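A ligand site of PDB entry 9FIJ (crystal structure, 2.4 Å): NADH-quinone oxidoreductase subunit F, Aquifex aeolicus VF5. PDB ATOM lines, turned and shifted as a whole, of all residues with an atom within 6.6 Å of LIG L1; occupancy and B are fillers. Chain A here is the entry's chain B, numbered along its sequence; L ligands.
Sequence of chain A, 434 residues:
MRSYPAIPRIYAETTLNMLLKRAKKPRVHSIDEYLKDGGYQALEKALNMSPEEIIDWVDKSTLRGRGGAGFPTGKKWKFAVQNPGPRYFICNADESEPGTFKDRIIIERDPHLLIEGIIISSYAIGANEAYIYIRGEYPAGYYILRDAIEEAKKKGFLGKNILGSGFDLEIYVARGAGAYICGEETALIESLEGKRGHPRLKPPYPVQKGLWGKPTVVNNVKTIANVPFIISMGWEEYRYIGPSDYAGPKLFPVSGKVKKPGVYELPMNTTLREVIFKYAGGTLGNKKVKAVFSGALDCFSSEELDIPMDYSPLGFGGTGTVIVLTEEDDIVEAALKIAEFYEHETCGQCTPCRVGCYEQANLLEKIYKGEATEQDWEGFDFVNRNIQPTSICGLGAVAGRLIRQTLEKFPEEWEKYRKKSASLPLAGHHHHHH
Ile 181 touches LIG L1 (CD1 to S4, 3.7 Å).
CG of Pro 199 touches S2 of LIG L1, 3.7 Å away.
Ser 391 touches LIG L1 (CB to S1, 3.5 Å).
Ile 392 touches LIG L1.
CB of Leu 395 touches S4 of LIG L1, at 3.9 Å.
Of the 25 residues printed, 13 come within 4 Å of LIG L1.
The nearest printed residue that does not touch LIG L1 is Arg 354 (4.7 Å).
A sulfur (S3) of LIG L1 sits close to the backbone NH (N) of Cys 350 (3.2 Å).
SG of Cys 350 is bound to FE4 of LIG L1 (2.3 Å).
The side-chain sulfur (SG) of Cys 393 is bound to an iron atom (FE3) of LIG L1 (2.3 Å).
A sulfur (S4) of LIG L1 sits close to the backbone NH of Cys 347, 3.6 Å away.
The side-chain sulfur (SG) of Cys 347 binds an iron atom (FE1) of LIG L1 (2.3 Å).
FE2 of LIG L1 is bound by SG of Cys 353 (2.3 Å).
The backbone NH (N) of Gln 349 lies close to a sulfur (S3) of LIG L1.
A sulfur (S2) of LIG L1 sits close to the side-chain amide oxygen (OE1) of Gln 349, at 3.5 Å.
The backbone NH of Gly 348 sits close to a sulfur (S3) of LIG L1.
The backbone NH of Gly 396 sits close to a sulfur (S1) of LIG L1, at 3.6 Å.
The side-chain hydroxyl (OG1) of Thr 346 sits close to a sulfur (S3) of LIG L1 (3.8 Å).
The backbone NH of Leu 395 sits close to the side-chain sulfur of Cys 393, at 3.6 Å.
SG of Cys 347 sits close to OE1 of Gln 349, 3.7 Å away.
The side-chain sulfur (SG) of Cys 353 sits close to the side-chain hydroxyl (OG1) of Thr 346 (3.0 Å).
The backbone carbonyl oxygen (O) of Cys 353 lies close to the side-chain sulfur (SG) of Cys 357 (3.4 Å).
The backbone carbonyl oxygen (O) of Ile 387 is in hydrogen-bond range of the backbone NH (N) of Cys 353, at 3.5 Å.
The side-chain amide oxygen of Gln 349 lies close to the backbone carbonyl oxygen of Pro 199.
OG of Ser 391 lies within hydrogen-bond range of O of Gln 388 (2.4 Å).
The backbone carbonyl oxygen (O) of Gly 348 is in hydrogen-bond range of the guanidinium group (NH1) of Arg 354 (3.1 Å).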
ATOM      1  N   ILE A 181     -20.643  18.336 -16.736  1.00  0.00           N
ATOM      2  CA  ILE A 181     -19.924  17.099 -17.014  1.00  0.00           C
ATOM      3  C   ILE A 181     -20.424  15.990 -16.097  1.00  0.00           C
ATOM      4  O   ILE A 181     -20.279  14.825 -16.450  1.00  0.00           O
ATOM      5  CB  ILE A 181     -18.395  17.261 -16.913  1.00  0.00           C
ATOM      6  CG1 ILE A 181     -17.658  16.074 -17.548  1.00  0.00           C
ATOM      7  CG2 ILE A 181     -17.932  17.477 -15.477  1.00  0.00           C
ATOM      8  CD1 ILE A 181     -17.987  15.833 -19.015  1.00  0.00           C
ATOM      9  N   GLY A 197     -16.024  15.799 -10.472  1.00  0.00           N
ATOM     10  CA  GLY A 197     -16.695  15.139 -11.573  1.00  0.00           C
ATOM     11  C   GLY A 197     -15.764  14.956 -12.776  1.00  0.00           C
ATOM     12  O   GLY A 197     -15.944  15.610 -13.794  1.00  0.00           O
ATOM     13  N   HIS A 198     -14.790  14.041 -12.634  1.00  0.00           N
ATOM     14  CA  HIS A 198     -13.865  13.702 -13.700  1.00  0.00           C
ATOM     15  C   HIS A 198     -14.309  12.378 -14.319  1.00  0.00           C
ATOM     16  O   HIS A 198     -14.334  11.359 -13.642  1.00  0.00           O
ATOM     17  CB  HIS A 198     -12.422  13.605 -13.175  1.00  0.00           C
ATOM     18  CG  HIS A 198     -11.777  14.914 -12.928  1.00  0.00           C
ATOM     19  ND1 HIS A 198     -10.760  15.091 -12.009  1.00  0.00           N
ATOM     20  CD2 HIS A 198     -11.975  16.125 -13.485  1.00  0.00           C
ATOM     21  CE1 HIS A 198     -10.374  16.354 -12.012  1.00  0.00           C
ATOM     22  NE2 HIS A 198     -11.091  17.002 -12.912  1.00  0.00           N
ATOM     23  N   PRO A 199     -14.684  12.348 -15.618  1.00  0.00           N
ATOM     24  CA  PRO A 199     -14.918  11.100 -16.331  1.00  0.00           C
ATOM     25  C   PRO A 199     -13.771  10.100 -16.300  1.00  0.00           C
ATOM     26  O   PRO A 199     -12.602  10.482 -16.407  1.00  0.00           O
ATOM     27  CB  PRO A 199     -15.211  11.556 -17.773  1.00  0.00           C
ATOM     28  CG  PRO A 199     -15.788  12.956 -17.601  1.00  0.00           C
ATOM     29  CD  PRO A 199     -15.002  13.528 -16.436  1.00  0.00           C
ATOM     30  N   ARG A 200     -14.145   8.815 -16.158  1.00  0.00           N
ATOM     31  CA  ARG A 200     -13.222   7.682 -16.142  1.00  0.00           C
ATOM     32  C   ARG A 200     -13.030   7.179 -17.568  1.00  0.00           C
ATOM     33  O   ARG A 200     -13.960   7.176 -18.367  1.00  0.00           O
ATOM     34  CB  ARG A 200     -13.766   6.470 -15.385  1.00  0.00           C
ATOM     35  CG  ARG A 200     -14.135   6.724 -13.925  1.00  0.00           C
ATOM     36  CD  ARG A 200     -14.881   5.535 -13.358  1.00  0.00           C
ATOM     37  NE  ARG A 200     -15.232   5.771 -11.946  1.00  0.00           N
ATOM     38  CZ  ARG A 200     -15.816   4.880 -11.150  1.00  0.00           C
ATOM     39  NH1 ARG A 200     -16.241   3.729 -11.624  1.00  0.00           N
ATOM     40  NH2 ARG A 200     -15.987   5.163  -9.860  1.00  0.00           N
ATOM     41  N   GLU A 345     -17.492  24.228 -19.201  1.00  0.00           N
ATOM     42  CA  GLU A 345     -17.909  22.895 -18.814  1.00  0.00           C
ATOM     43  C   GLU A 345     -16.825  21.819 -18.987  1.00  0.00           C
ATOM     44  O   GLU A 345     -16.942  20.760 -18.366  1.00  0.00           O
ATOM     45  CB  GLU A 345     -19.211  22.555 -19.540  1.00  0.00           C
ATOM     46  CG  GLU A 345     -20.369  23.465 -19.134  1.00  0.00           C
ATOM     47  CD  GLU A 345     -20.710  23.625 -17.656  1.00  0.00           C
ATOM     48  OE1 GLU A 345     -20.147  22.907 -16.778  1.00  0.00           O
ATOM     49  OE2 GLU A 345     -21.539  24.508 -17.356  1.00  0.00           O
ATOM     50  N   THR A 346     -15.796  22.063 -19.809  1.00  0.00           N
ATOM     51  CA  THR A 346     -14.695  21.110 -19.923  1.00  0.00           C
ATOM     52  C   THR A 346     -14.142  20.831 -18.523  1.00  0.00           C
ATOM     53  O   THR A 346     -13.916  21.760 -17.741  1.00  0.00           O
ATOM     54  CB  THR A 346     -13.617  21.618 -20.887  1.00  0.00           C
ATOM     55  OG1 THR A 346     -12.599  20.604 -20.932  1.00  0.00           O
ATOM     56  CG2 THR A 346     -12.973  22.935 -20.473  1.00  0.00           C
ATOM     57  N   CYS A 347     -13.912  19.562 -18.197  1.00  0.00           N
ATOM     58  CA  CYS A 347     -13.408  19.215 -16.872  1.00  0.00           C
ATOM     59  C   CYS A 347     -11.905  19.468 -16.775  1.00  0.00           C
ATOM     60  O   CYS A 347     -11.404  19.636 -15.663  1.00  0.00           O
ATOM     61  CB  CYS A 347     -13.794  17.805 -16.429  1.00  0.00           C
ATOM     62  SG  CYS A 347     -12.793  16.465 -17.127  1.00  0.00           S
ATOM     63  N   GLY A 348     -11.198  19.450 -17.912  1.00  0.00           N
ATOM     64  CA  GLY A 348      -9.806  19.867 -17.983  1.00  0.00           C
ATOM     65  C   GLY A 348      -8.815  18.705 -18.032  1.00  0.00           C
ATOM     66  O   GLY A 348      -7.622  18.945 -18.135  1.00  0.00           O
ATOM     67  N   GLN A 349      -9.294  17.457 -17.941  1.00  0.00           N
ATOM     68  CA  GLN A 349      -8.432  16.282 -17.820  1.00  0.00           C
ATOM     69  C   GLN A 349      -7.583  16.072 -19.065  1.00  0.00           C
ATOM     70  O   GLN A 349      -6.434  15.654 -18.963  1.00  0.00           O
ATOM     71  CB  GLN A 349      -9.246  14.991 -17.684  1.00  0.00           C
ATOM     72  CG  GLN A 349      -9.530  14.551 -16.253  1.00  0.00           C
ATOM     73  CD  GLN A 349     -10.270  13.230 -16.220  1.00  0.00           C
ATOM     74  OE1 GLN A 349     -11.378  13.096 -16.750  1.00  0.00           O
ATOM     75  NE2 GLN A 349      -9.642  12.234 -15.610  1.00  0.00           N
ATOM     76  N   CYS A 350      -8.196  16.268 -20.244  1.00  0.00           N
ATOM     77  CA  CYS A 350      -7.553  16.040 -21.525  1.00  0.00           C
ATOM     78  C   CYS A 350      -7.087  17.391 -22.062  1.00  0.00           C
ATOM     79  O   CYS A 350      -7.782  18.392 -21.909  1.00  0.00           O
ATOM     80  CB  CYS A 350      -8.511  15.359 -22.499  1.00  0.00           C
ATOM     81  SG  CYS A 350      -9.580  14.117 -21.732  1.00  0.00           S
ATOM     82  N   THR A 351      -5.890  17.426 -22.659  1.00  0.00           N
ATOM     83  CA  THR A 351      -5.256  18.696 -22.951  1.00  0.00           C
ATOM     84  C   THR A 351      -5.970  19.356 -24.132  1.00  0.00           C
ATOM     85  O   THR A 351      -6.311  20.543 -24.078  1.00  0.00           O
ATOM     86  CB  THR A 351      -3.754  18.480 -23.169  1.00  0.00           C
ATOM     87  OG1 THR A 351      -3.193  18.507 -21.855  1.00  0.00           O
ATOM     88  CG2 THR A 351      -3.106  19.579 -23.980  1.00  0.00           C
ATOM     89  N   CYS A 353      -9.010  19.152 -25.151  1.00  0.00           N
ATOM     90  CA  CYS A 353     -10.315  19.617 -24.731  1.00  0.00           C
ATOM     91  C   CYS A 353     -10.180  20.855 -23.838  1.00  0.00           C
ATOM     92  O   CYS A 353     -10.843  21.868 -24.064  1.00  0.00           O
ATOM     93  CB  CYS A 353     -11.088  18.475 -24.073  1.00  0.00           C
ATOM     94  SG  CYS A 353     -12.724  18.905 -23.406  1.00  0.00           S
ATOM     95  N   ARG A 354      -9.316  20.746 -22.822  1.00  0.00           N
ATOM     96  CA  ARG A 354      -9.076  21.833 -21.881  1.00  0.00           C
ATOM     97  C   ARG A 354      -8.739  23.109 -22.648  1.00  0.00           C
ATOM     98  O   ARG A 354      -9.365  24.157 -22.455  1.00  0.00           O
ATOM     99  CB  ARG A 354      -7.912  21.470 -20.942  1.00  0.00           C
ATOM    100  CG  ARG A 354      -7.482  22.549 -19.959  1.00  0.00           C
ATOM    101  CD  ARG A 354      -6.452  22.060 -18.952  1.00  0.00           C
ATOM    102  NE  ARG A 354      -5.111  21.978 -19.538  1.00  0.00           N
ATOM    103  CZ  ARG A 354      -4.503  20.848 -19.906  1.00  0.00           C
ATOM    104  NH1 ARG A 354      -5.134  19.673 -19.781  1.00  0.00           N
ATOM    105  NH2 ARG A 354      -3.289  20.907 -20.408  1.00  0.00           N
ATOM    106  N   CYS A 357     -11.411  24.112 -25.814  1.00  0.00           N
ATOM    107  CA  CYS A 357     -12.688  24.693 -25.418  1.00  0.00           C
ATOM    108  C   CYS A 357     -12.473  26.162 -25.038  1.00  0.00           C
ATOM    109  O   CYS A 357     -13.264  27.023 -25.426  1.00  0.00           O
ATOM    110  CB  CYS A 357     -13.372  23.907 -24.302  1.00  0.00           C
ATOM    111  SG  CYS A 357     -14.114  22.322 -24.806  1.00  0.00           S
ATOM    112  N   ILE A 387     -10.262  19.795 -30.901  1.00  0.00           N
ATOM    113  CA  ILE A 387     -10.667  19.665 -29.521  1.00  0.00           C
ATOM    114  C   ILE A 387     -10.743  18.183 -29.150  1.00  0.00           C
ATOM    115  O   ILE A 387     -10.564  17.823 -27.987  1.00  0.00           O
ATOM    116  CB  ILE A 387     -12.015  20.376 -29.268  1.00  0.00           C
ATOM    117  CG1 ILE A 387     -11.989  21.826 -29.751  1.00  0.00           C
ATOM    118  CG2 ILE A 387     -12.414  20.275 -27.798  1.00  0.00           C
ATOM    119  CD1 ILE A 387     -13.279  22.612 -29.503  1.00  0.00           C
ATOM    120  N   GLN A 388     -10.999  17.329 -30.148  1.00  0.00           N
ATOM    121  CA  GLN A 388     -11.335  15.929 -29.935  1.00  0.00           C
ATOM    122  C   GLN A 388     -10.132  15.080 -29.507  1.00  0.00           C
ATOM    123  O   GLN A 388     -10.254  14.279 -28.581  1.00  0.00           O
ATOM    124  CB  GLN A 388     -11.998  15.348 -31.192  1.00  0.00           C
ATOM    125  CG  GLN A 388     -11.742  13.856 -31.358  1.00  0.00           C
ATOM    126  CD  GLN A 388     -12.895  13.092 -31.975  1.00  0.00           C
ATOM    127  OE1 GLN A 388     -13.982  13.637 -32.220  1.00  0.00           O
ATOM    128  NE2 GLN A 388     -12.683  11.813 -32.196  1.00  0.00           N
ATOM    129  N   THR A 390      -7.388  12.586 -28.199  1.00  0.00           N
ATOM    130  CA  THR A 390      -6.983  12.083 -26.897  1.00  0.00           C
ATOM    131  C   THR A 390      -8.084  12.188 -25.846  1.00  0.00           C
ATOM    132  O   THR A 390      -7.844  11.824 -24.693  1.00  0.00           O
ATOM    133  CB  THR A 390      -5.710  12.783 -26.395  1.00  0.00           C
ATOM    134  OG1 THR A 390      -6.072  14.049 -25.841  1.00  0.00           O
ATOM    135  CG2 THR A 390      -4.646  12.874 -27.476  1.00  0.00           C
ATOM    136  N   SER A 391      -9.287  12.647 -26.237  1.00  0.00           N
ATOM    137  CA  SER A 391     -10.370  12.872 -25.287  1.00  0.00           C
ATOM    138  C   SER A 391     -10.961  11.542 -24.815  1.00  0.00           C
ATOM    139  O   SER A 391     -11.077  10.617 -25.614  1.00  0.00           O
ATOM    140  CB  SER A 391     -11.445  13.765 -25.858  1.00  0.00           C
ATOM    141  OG  SER A 391     -11.906  13.304 -27.128  1.00  0.00           O
ATOM    142  N   ILE A 392     -11.370  11.474 -23.541  1.00  0.00           N
ATOM    143  CA  ILE A 392     -11.858  10.221 -22.965  1.00  0.00           C
ATOM    144  C   ILE A 392     -13.368  10.258 -22.729  1.00  0.00           C
ATOM    145  O   ILE A 392     -13.891   9.332 -22.142  1.00  0.00           O
ATOM    146  CB  ILE A 392     -11.099   9.860 -21.667  1.00  0.00           C
ATOM    147  CG1 ILE A 392     -11.256  10.920 -20.582  1.00  0.00           C
ATOM    148  CG2 ILE A 392      -9.631   9.563 -21.949  1.00  0.00           C
ATOM    149  CD1 ILE A 392     -10.550  10.572 -19.281  1.00  0.00           C
ATOM    150  N   CYS A 393     -14.055  11.322 -23.153  1.00  0.00           N
ATOM    151  CA  CYS A 393     -15.502  11.387 -23.024  1.00  0.00           C
ATOM    152  C   CYS A 393     -16.106  12.215 -24.154  1.00  0.00           C
ATOM    153  O   CYS A 393     -15.401  12.826 -24.944  1.00  0.00           O
ATOM    154  CB  CYS A 393     -15.920  11.917 -21.653  1.00  0.00           C
ATOM    155  SG  CYS A 393     -16.241  13.696 -21.608  1.00  0.00           S
ATOM    156  N   GLY A 394     -17.444  12.220 -24.216  1.00  0.00           N
ATOM    157  CA  GLY A 394     -18.156  12.698 -25.388  1.00  0.00           C
ATOM    158  C   GLY A 394     -18.045  14.215 -25.600  1.00  0.00           C
ATOM    159  O   GLY A 394     -18.155  14.668 -26.731  1.00  0.00           O
ATOM    160  N   LEU A 395     -17.835  14.977 -24.522  1.00  0.00           N
ATOM    161  CA  LEU A 395     -17.830  16.434 -24.603  1.00  0.00           C
ATOM    162  C   LEU A 395     -16.750  16.935 -25.562  1.00  0.00           C
ATOM    163  O   LEU A 395     -17.005  17.801 -26.400  1.00  0.00           O
ATOM    164  CB  LEU A 395     -17.662  17.026 -23.204  1.00  0.00           C
ATOM    165  CG  LEU A 395     -17.766  18.543 -23.094  1.00  0.00           C
ATOM    166  CD1 LEU A 395     -18.184  18.980 -21.693  1.00  0.00           C
ATOM    167  CD2 LEU A 395     -16.462  19.234 -23.487  1.00  0.00           C
ATOM    168  N   GLY A 396     -15.523  16.403 -25.401  1.00  0.00           N
ATOM    169  CA  GLY A 396     -14.419  16.769 -26.275  1.00  0.00           C
ATOM    170  C   GLY A 396     -14.724  16.457 -27.728  1.00  0.00           C
ATOM    171  O   GLY A 396     -14.367  17.223 -28.630  1.00  0.00           O
ATOM    172  N   ALA A 397     -15.423  15.349 -27.973  1.00  0.00           N
ATOM    173  CA  ALA A 397     -15.736  14.917 -29.326  1.00  0.00           C
ATOM    174  C   ALA A 397     -16.748  15.838 -30.004  1.00  0.00           C
ATOM    175  O   ALA A 397     -16.851  15.776 -31.219  1.00  0.00           O
ATOM    176  CB  ALA A 397     -16.241  13.485 -29.287  1.00  0.00           C
HETATM  177 FE1  LIG L   1     -12.985  16.271 -19.382  1.00  0.00          FE
HETATM  178 FE2  LIG L   1     -13.089  17.173 -21.951  1.00  0.00          FE
HETATM  179 FE3  LIG L   1     -14.341  14.898 -21.286  1.00  0.00          FE
HETATM  180 FE4  LIG L   1     -11.626  14.969 -21.307  1.00  0.00          FE
HETATM  181  S1  LIG L   1     -13.032  15.217 -23.102  1.00  0.00           S
HETATM  182  S2  LIG L   1     -12.929  14.031 -19.722  1.00  0.00           S
HETATM  183  S3  LIG L   1     -11.265  17.090 -20.586  1.00  0.00           S
HETATM  184  S4  LIG L   1     -14.817  16.969 -20.539  1.00  0.00           S
HETATM  185  C1  LG2 L   2     -24.305  12.837 -20.879  1.00  0.00           C
HETATM  186  N1  LG2 L   2     -25.405  11.944 -20.612  1.00  0.00           N
HETATM  187  C2  LG2 L   2     -26.486  12.451 -19.902  1.00  0.00           C
HETATM  188  N2  LG2 L   2     -27.502  11.594 -19.563  1.00  0.00           N
HETATM  189  C3  LG2 L   2     -28.548  11.966 -18.755  1.00  0.00           C
HETATM  190  O1  LG2 L   2     -29.389  11.154 -18.349  1.00  0.00           O
HETATM  191  N3  LG2 L   2     -28.565  13.293 -18.383  1.00  0.00           N
HETATM  192  C4  LG2 L   2     -27.604  14.258 -18.690  1.00  0.00           C
HETATM  193  O2  LG2 L   2     -27.722  15.419 -18.284  1.00  0.00           O
HETATM  194  C5  LG2 L   2     -26.534  13.762 -19.469  1.00  0.00           C
HETATM  195  N4  LG2 L   2     -25.489  14.584 -19.710  1.00  0.00           N
HETATM  196  C6  LG2 L   2     -24.364  14.149 -20.373  1.00  0.00           C
HETATM  197  C7  LG2 L   2     -23.297  15.013 -20.545  1.00  0.00           C
HETATM  198  C8  LG2 L   2     -22.148  14.606 -21.229  1.00  0.00           C
HETATM  199  C9  LG2 L   2     -21.006  15.580 -21.382  1.00  0.00           C
HETATM  200  C10 LG2 L   2     -22.081  13.304 -21.742  1.00  0.00           C
HETATM  201  C11 LG2 L   2     -20.876  12.851 -22.528  1.00  0.00           C
HETATM  202  C12 LG2 L   2     -23.156  12.431 -21.563  1.00  0.00           C
HETATM  203  C13 LG2 L   2     -25.360  10.543 -21.028  1.00  0.00           C
HETATM  204  C14 LG2 L   2     -25.022   9.625 -19.857  1.00  0.00           C
HETATM  205  O3  LG2 L   2     -23.598   9.515 -19.744  1.00  0.00           O
HETATM  206  C15 LG2 L   2     -25.607   8.225 -20.076  1.00  0.00           C
HETATM  207  O4  LG2 L   2     -25.453   7.819 -21.425  1.00  0.00           O
HETATM  208  C16 LG2 L   2     -27.099   8.111 -19.742  1.00  0.00           C
HETATM  209  O5  LG2 L   2     -27.430   8.789 -18.528  1.00  0.00           O
HETATM  210  C17 LG2 L   2     -27.519   6.669 -19.609  1.00  0.00           C
HETATM  211  O6  LG2 L   2     -28.929   6.644 -19.390  1.00  0.00           O
HETATM  212  P1  LG2 L   2     -29.898   6.060 -20.558  1.00  0.00           P
HETATM  213  O7  LG2 L   2     -29.355   4.722 -20.997  1.00  0.00           O
HETATM  214  O8  LG2 L   2     -31.219   5.967 -19.820  1.00  0.00           O
HETATM  215  O9  LG2 L   2     -29.930   7.069 -21.697  1.00  0.00           O
